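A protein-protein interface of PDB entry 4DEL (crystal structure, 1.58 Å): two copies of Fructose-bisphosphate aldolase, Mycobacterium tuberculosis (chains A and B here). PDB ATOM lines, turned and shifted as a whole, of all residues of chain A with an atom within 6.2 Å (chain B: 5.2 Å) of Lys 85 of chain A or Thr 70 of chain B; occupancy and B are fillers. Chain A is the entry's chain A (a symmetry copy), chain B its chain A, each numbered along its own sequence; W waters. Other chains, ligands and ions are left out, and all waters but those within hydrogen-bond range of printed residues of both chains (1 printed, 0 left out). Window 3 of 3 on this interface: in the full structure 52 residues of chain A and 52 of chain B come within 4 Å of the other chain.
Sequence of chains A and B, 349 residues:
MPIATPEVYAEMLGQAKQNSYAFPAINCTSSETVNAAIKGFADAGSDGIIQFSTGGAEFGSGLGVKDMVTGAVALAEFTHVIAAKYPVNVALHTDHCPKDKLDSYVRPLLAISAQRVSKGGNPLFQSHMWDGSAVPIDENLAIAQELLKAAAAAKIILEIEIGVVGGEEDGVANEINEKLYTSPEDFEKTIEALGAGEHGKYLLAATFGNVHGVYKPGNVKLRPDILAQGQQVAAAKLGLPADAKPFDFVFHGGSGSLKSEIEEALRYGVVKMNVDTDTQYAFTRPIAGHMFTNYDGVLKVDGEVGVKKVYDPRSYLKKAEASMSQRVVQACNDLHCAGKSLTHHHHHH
N of Asp 67 of chain B sits at hydrogen-bond distance from OG of Ser 61 of chain B, 2.9 Å away.
The side-chain hydroxyl (OG1) of Thr 70 of chain B sits at hydrogen-bond distance from the side-chain carboxylate (OD2) of Asp 67 of chain B, 2.8 Å away.
Among the printed residues, pairs that only touch across the chains: Val 81 of chain A with Thr 70 of chain B (3.7 Å), Val 81 of chain A with Ala 74 of chain B (3.7 Å), Ile 82 of chain A with Ser 61 of chain B (3.8 Å), Ile 82 of chain A with Thr 70 of chain B (3.9 Å), Ile 82 of chain A with Ala 74 of chain B (3.9 Å), Lys 85 of chain A with Thr 70 of chain B (3.5 Å) and Tyr 86 of chain A with Val 65 of chain B (3.4 Å).
Of the printed residues of chain B, Tyr 86 of chain A touches Val 65.
Pro 87 of chain A touches none of the printed residues of chain B.
Printed residues of chain A within 4 Å of Ala 74 of chain B: Val 81 and Ile 82.
The nearest residue of chain B that does not touch Lys 85 of chain A is Val 65 of chain B (4.1 Å).
The nearest printed residue of chain A that does not touch Thr 70 of chain B is Ala 83 of chain A (6.6 Å).
The nearest printed residue of chain A that does not touch Val 65 of chain B is Lys 85 of chain A (4.1 Å).
Printed residues of chain A that touch a printed residue of chain B: Val 81, Ile 82, Lys 85 and Tyr 86.
Hydrophobic or aromatic side chains of chain A within 4 Å of the printed part of chain B: Val 81, Ile 82 and Tyr 86.
Of the 11 printed residues of chain B, 4 touch a printed residue of chain A.
Printed residues of chain B that touch a printed residue of chain A: Ser 61, Val 65, Thr 70 and Ala 74.
Hydrophobic or aromatic side chains of chain B that line the printed part of chain A: Val 65 and Ala 74.
Among the printed residues, no Asp or Glu carboxylate lies within 4 Å of a Lys or Arg side-chain nitrogen of the other chain.
No position is printed for both chains.
Water W1 bridges the side-chain hydroxyl (OH) of Tyr 86 of chain A and the backbone carbonyl oxygen (O) of Ser 61 of chain B.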
ATOM      1  N   PRO A   2      17.039 -10.632  20.237  1.00  0.00           N
ATOM      2  CA  PRO A   2      16.597 -11.645  21.196  1.00  0.00           C
ATOM      3  C   PRO A   2      17.689 -12.656  21.494  1.00  0.00           C
ATOM      4  O   PRO A   2      18.653 -12.741  20.745  1.00  0.00           O
ATOM      5  CB  PRO A   2      15.456 -12.361  20.440  1.00  0.00           C
ATOM      6  CG  PRO A   2      15.738 -12.078  18.978  1.00  0.00           C
ATOM      7  CD  PRO A   2      16.234 -10.674  19.000  1.00  0.00           C
ATOM      8  N   HIS A  80      19.698 -12.326  29.176  1.00  0.00           N
ATOM      9  CA  HIS A  80      18.351 -12.592  28.630  1.00  0.00           C
ATOM     10  C   HIS A  80      17.482 -11.333  28.607  1.00  0.00           C
ATOM     11  O   HIS A  80      16.746 -11.083  27.635  1.00  0.00           O
ATOM     12  CB  HIS A  80      17.629 -13.703  29.403  1.00  0.00           C
ATOM     13  CG  HIS A  80      18.045 -15.087  29.009  1.00  0.00           C
ATOM     14  ND1 HIS A  80      17.209 -15.954  28.334  1.00  0.00           N
ATOM     15  CD2 HIS A  80      19.208 -15.752  29.189  1.00  0.00           C
ATOM     16  CE1 HIS A  80      17.835 -17.101  28.135  1.00  0.00           C
ATOM     17  NE2 HIS A  80      19.053 -17.005  28.635  1.00  0.00           N
ATOM     18  N   VAL A  81      17.557 -10.528  29.670  1.00  0.00           N
ATOM     19  CA  VAL A  81      16.805  -9.280  29.709  1.00  0.00           C
ATOM     20  C   VAL A  81      17.303  -8.304  28.641  1.00  0.00           C
ATOM     21  O   VAL A  81      16.502  -7.752  27.874  1.00  0.00           O
ATOM     22  CB  VAL A  81      16.842  -8.645  31.123  1.00  0.00           C
ATOM     23  CG1 VAL A  81      16.073  -7.320  31.148  1.00  0.00           C
ATOM     24  CG2 VAL A  81      16.310  -9.652  32.149  1.00  0.00           C
ATOM     25  N   ILE A  82      18.620  -8.097  28.573  1.00  0.00           N
ATOM     26  CA  ILE A  82      19.189  -7.141  27.614  1.00  0.00           C
ATOM     27  C   ILE A  82      18.919  -7.549  26.161  1.00  0.00           C
ATOM     28  O   ILE A  82      18.462  -6.723  25.357  1.00  0.00           O
ATOM     29  CB  ILE A  82      20.711  -6.937  27.856  1.00  0.00           C
ATOM     30  CG1 ILE A  82      20.961  -6.329  29.258  1.00  0.00           C
ATOM     31  CG2 ILE A  82      21.342  -6.085  26.741  1.00  0.00           C
ATOM     32  CD1 ILE A  82      20.266  -4.985  29.525  1.00  0.00           C
ATOM     33  N   ALA A  83      19.185  -8.813  25.841  1.00  0.00           N
ATOM     34  CA  ALA A  83      19.162  -9.284  24.445  1.00  0.00           C
ATOM     35  C   ALA A  83      17.761  -9.174  23.836  1.00  0.00           C
ATOM     36  O   ALA A  83      17.617  -8.997  22.633  1.00  0.00           O
ATOM     37  CB  ALA A  83      19.716 -10.704  24.334  1.00  0.00           C
ATOM     38  N   ALA A  84      16.731  -9.260  24.681  1.00  0.00           N
ATOM     39  CA  ALA A  84      15.346  -9.080  24.213  1.00  0.00           C
ATOM     40  C   ALA A  84      15.097  -7.709  23.564  1.00  0.00           C
ATOM     41  O   ALA A  84      14.143  -7.546  22.796  1.00  0.00           O
ATOM     42  CB  ALA A  84      14.352  -9.320  25.364  1.00  0.00           C
ATOM     43  N   LYS A  85      15.938  -6.718  23.873  1.00  0.00           N
ATOM     44  CA  LYS A  85      15.766  -5.348  23.377  1.00  0.00           C
ATOM     45  C   LYS A  85      16.616  -5.038  22.142  1.00  0.00           C
ATOM     46  O   LYS A  85      16.655  -3.884  21.685  1.00  0.00           O
ATOM     47  CB  LYS A  85      16.087  -4.324  24.488  1.00  0.00           C
ATOM     48  CG  LYS A  85      15.265  -4.500  25.751  1.00  0.00           C
ATOM     49  CD  LYS A  85      13.790  -4.247  25.512  1.00  0.00           C
ATOM     50  CE  LYS A  85      13.496  -2.755  25.405  1.00  0.00           C
ATOM     51  NZ  LYS A  85      12.048  -2.517  25.149  1.00  0.00           N
ATOM     52  N   TYR A  86      17.287  -6.053  21.597  1.00  0.00           N
ATOM     53  CA  TYR A  86      18.089  -5.867  20.376  1.00  0.00           C
ATOM     54  C   TYR A  86      17.547  -6.709  19.224  1.00  0.00           C
ATOM     55  O   TYR A  86      17.127  -7.840  19.464  1.00  0.00           O
ATOM     56  CB  TYR A  86      19.536  -6.278  20.624  1.00  0.00           C
ATOM     57  CG  TYR A  86      20.361  -5.286  21.400  1.00  0.00           C
ATOM     58  CD1 TYR A  86      21.074  -4.286  20.744  1.00  0.00           C
ATOM     59  CD2 TYR A  86      20.473  -5.377  22.797  1.00  0.00           C
ATOM     60  CE1 TYR A  86      21.862  -3.376  21.434  1.00  0.00           C
ATOM     61  CE2 TYR A  86      21.271  -4.480  23.497  1.00  0.00           C
ATOM     62  CZ  TYR A  86      21.957  -3.479  22.812  1.00  0.00           C
ATOM     63  OH  TYR A  86      22.759  -2.584  23.481  1.00  0.00           O
ATOM     64  N   PRO A  87      17.600  -6.194  17.982  1.00  0.00           N
ATOM     65  CA  PRO A  87      16.977  -6.974  16.906  1.00  0.00           C
ATOM     66  C   PRO A  87      17.753  -8.244  16.531  1.00  0.00           C
ATOM     67  O   PRO A  87      17.174  -9.154  15.950  1.00  0.00           O
ATOM     68  CB  PRO A  87      16.933  -5.988  15.735  1.00  0.00           C
ATOM     69  CG  PRO A  87      18.030  -5.019  15.998  1.00  0.00           C
ATOM     70  CD  PRO A  87      18.204  -4.940  17.495  1.00  0.00           C
ATOM     71  N   SER B  61      21.375  -0.638  31.218  1.00  0.00           N
ATOM     72  CA  SER B  61      20.714  -1.177  30.013  1.00  0.00           C
ATOM     73  C   SER B  61      21.641  -1.160  28.802  1.00  0.00           C
ATOM     74  O   SER B  61      21.341  -1.786  27.790  1.00  0.00           O
ATOM     75  CB  SER B  61      19.422  -0.407  29.682  1.00  0.00           C
ATOM     76  OG  SER B  61      19.685   0.851  29.102  1.00  0.00           O
ATOM     77  N   VAL B  65      20.577   0.519  24.224  1.00  0.00           N
ATOM     78  CA  VAL B  65      19.199   0.392  24.696  1.00  0.00           C
ATOM     79  C   VAL B  65      18.746   1.689  25.371  1.00  0.00           C
ATOM     80  O   VAL B  65      17.732   2.273  24.987  1.00  0.00           O
ATOM     81  CB  VAL B  65      19.026  -0.797  25.678  1.00  0.00           C
ATOM     82  CG1 VAL B  65      17.580  -0.889  26.136  1.00  0.00           C
ATOM     83  CG2 VAL B  65      19.454  -2.110  25.039  1.00  0.00           C
ATOM     84  N   ASP B  67      17.308   2.326  28.261  1.00  0.00           N
ATOM     85  CA  ASP B  67      15.939   2.204  28.765  1.00  0.00           C
ATOM     86  C   ASP B  67      16.003   1.897  30.247  1.00  0.00           C
ATOM     87  O   ASP B  67      16.574   0.872  30.645  1.00  0.00           O
ATOM     88  CB  ASP B  67      15.178   1.096  28.038  1.00  0.00           C
ATOM     89  CG  ASP B  67      13.734   0.996  28.499  1.00  0.00           C
ATOM     90  OD1 ASP B  67      12.936   1.894  28.152  1.00  0.00           O
ATOM     91  OD2 ASP B  67      13.417   0.039  29.220  1.00  0.00           O
ATOM     92  N   MET B  68      15.419   2.785  31.052  1.00  0.00           N
ATOM     93  CA  MET B  68      15.467   2.643  32.514  1.00  0.00           C
ATOM     94  C   MET B  68      14.846   1.347  33.033  1.00  0.00           C
ATOM     95  O   MET B  68      15.418   0.685  33.901  1.00  0.00           O
ATOM     96  CB  MET B  68      14.803   3.841  33.196  1.00  0.00           C
ATOM     97  CG  MET B  68      15.524   5.153  32.966  1.00  0.00           C
ATOM     98  SD  MET B  68      14.599   6.493  33.726  1.00  0.00           S
ATOM     99  CE  MET B  68      13.208   6.656  32.609  1.00  0.00           C
ATOM    100  N   VAL B  69      13.676   0.981  32.513  1.00  0.00           N
ATOM    101  CA  VAL B  69      13.033  -0.266  32.939  1.00  0.00           C
ATOM    102  C   VAL B  69      13.900  -1.481  32.625  1.00  0.00           C
ATOM    103  O   VAL B  69      14.128  -2.323  33.486  1.00  0.00           O
ATOM    104  CB  VAL B  69      11.617  -0.414  32.354  1.00  0.00           C
ATOM    105  CG1 VAL B  69      11.066  -1.794  32.637  1.00  0.00           C
ATOM    106  CG2 VAL B  69      10.709   0.669  32.959  1.00  0.00           C
ATOM    107  N   THR B  70      14.412  -1.557  31.394  1.00  0.00           N
ATOM    108  CA  THR B  70      15.284  -2.665  31.023  1.00  0.00           C
ATOM    109  C   THR B  70      16.504  -2.800  31.962  1.00  0.00           C
ATOM    110  O   THR B  70      16.832  -3.894  32.417  1.00  0.00           O
ATOM    111  CB  THR B  70      15.752  -2.522  29.566  1.00  0.00           C
ATOM    112  OG1 THR B  70      14.600  -2.474  28.715  1.00  0.00           O
ATOM    113  CG2 THR B  70      16.626  -3.707  29.166  1.00  0.00           C
ATOM    114  N   GLY B  71      17.174  -1.683  32.241  1.00  0.00           N
ATOM    115  CA  GLY B  71      18.383  -1.703  33.066  1.00  0.00           C
ATOM    116  C   GLY B  71      18.093  -2.117  34.494  1.00  0.00           C
ATOM    117  O   GLY B  71      18.826  -2.937  35.082  1.00  0.00           O
ATOM    118  N   ALA B  72      17.018  -1.560  35.055  1.00  0.00           N
ATOM    119  CA  ALA B  72      16.618  -1.897  36.421  1.00  0.00           C
ATOM    120  C   ALA B  72      16.207  -3.372  36.531  1.00  0.00           C
ATOM    121  O   ALA B  72      16.576  -4.063  37.476  1.00  0.00           O
ATOM    122  CB  ALA B  72      15.489  -0.963  36.907  1.00  0.00           C
ATOM    123  N   VAL B  73      15.448  -3.870  35.558  1.00  0.00           N
ATOM    124  CA  VAL B  73      15.044  -5.274  35.582  1.00  0.00           C
ATOM    125  C   VAL B  73      16.258  -6.196  35.416  1.00  0.00           C
ATOM    126  O   VAL B  73      16.411  -7.178  36.131  1.00  0.00           O
ATOM    127  CB  VAL B  73      13.985  -5.586  34.487  1.00  0.00           C
ATOM    128  CG1 VAL B  73      13.728  -7.078  34.396  1.00  0.00           C
ATOM    129  CG2 VAL B  73      12.685  -4.815  34.751  1.00  0.00           C
ATOM    130  N   ALA B  74      17.123  -5.881  34.454  1.00  0.00           N
ATOM    131  CA  ALA B  74      18.309  -6.701  34.227  1.00  0.00           C
ATOM    132  C   ALA B  74      19.209  -6.762  35.471  1.00  0.00           C
ATOM    133  O   ALA B  74      19.660  -7.846  35.880  1.00  0.00           O
ATOM    134  CB  ALA B  74      19.086  -6.164  33.010  1.00  0.00           C
ATOM    135  N   LEU B  75      19.485  -5.602  36.057  1.00  0.00           N
ATOM    136  CA  LEU B  75      20.307  -5.555  37.271  1.00  0.00           C
ATOM    137  C   LEU B  75      19.599  -6.215  38.451  1.00  0.00           C
ATOM    138  O   LEU B  75      20.257  -6.865  39.268  1.00  0.00           O
ATOM    139  CB  LEU B  75      20.713  -4.115  37.604  1.00  0.00           C
ATOM    140  CG  LEU B  75      21.756  -3.493  36.659  1.00  0.00           C
ATOM    141  CD1 LEU B  75      21.914  -2.019  37.016  1.00  0.00           C
ATOM    142  CD2 LEU B  75      23.101  -4.238  36.680  1.00  0.00           C
HETATM  143  O   HOH W   1      22.837  -3.222  26.070  1.00  0.00           O
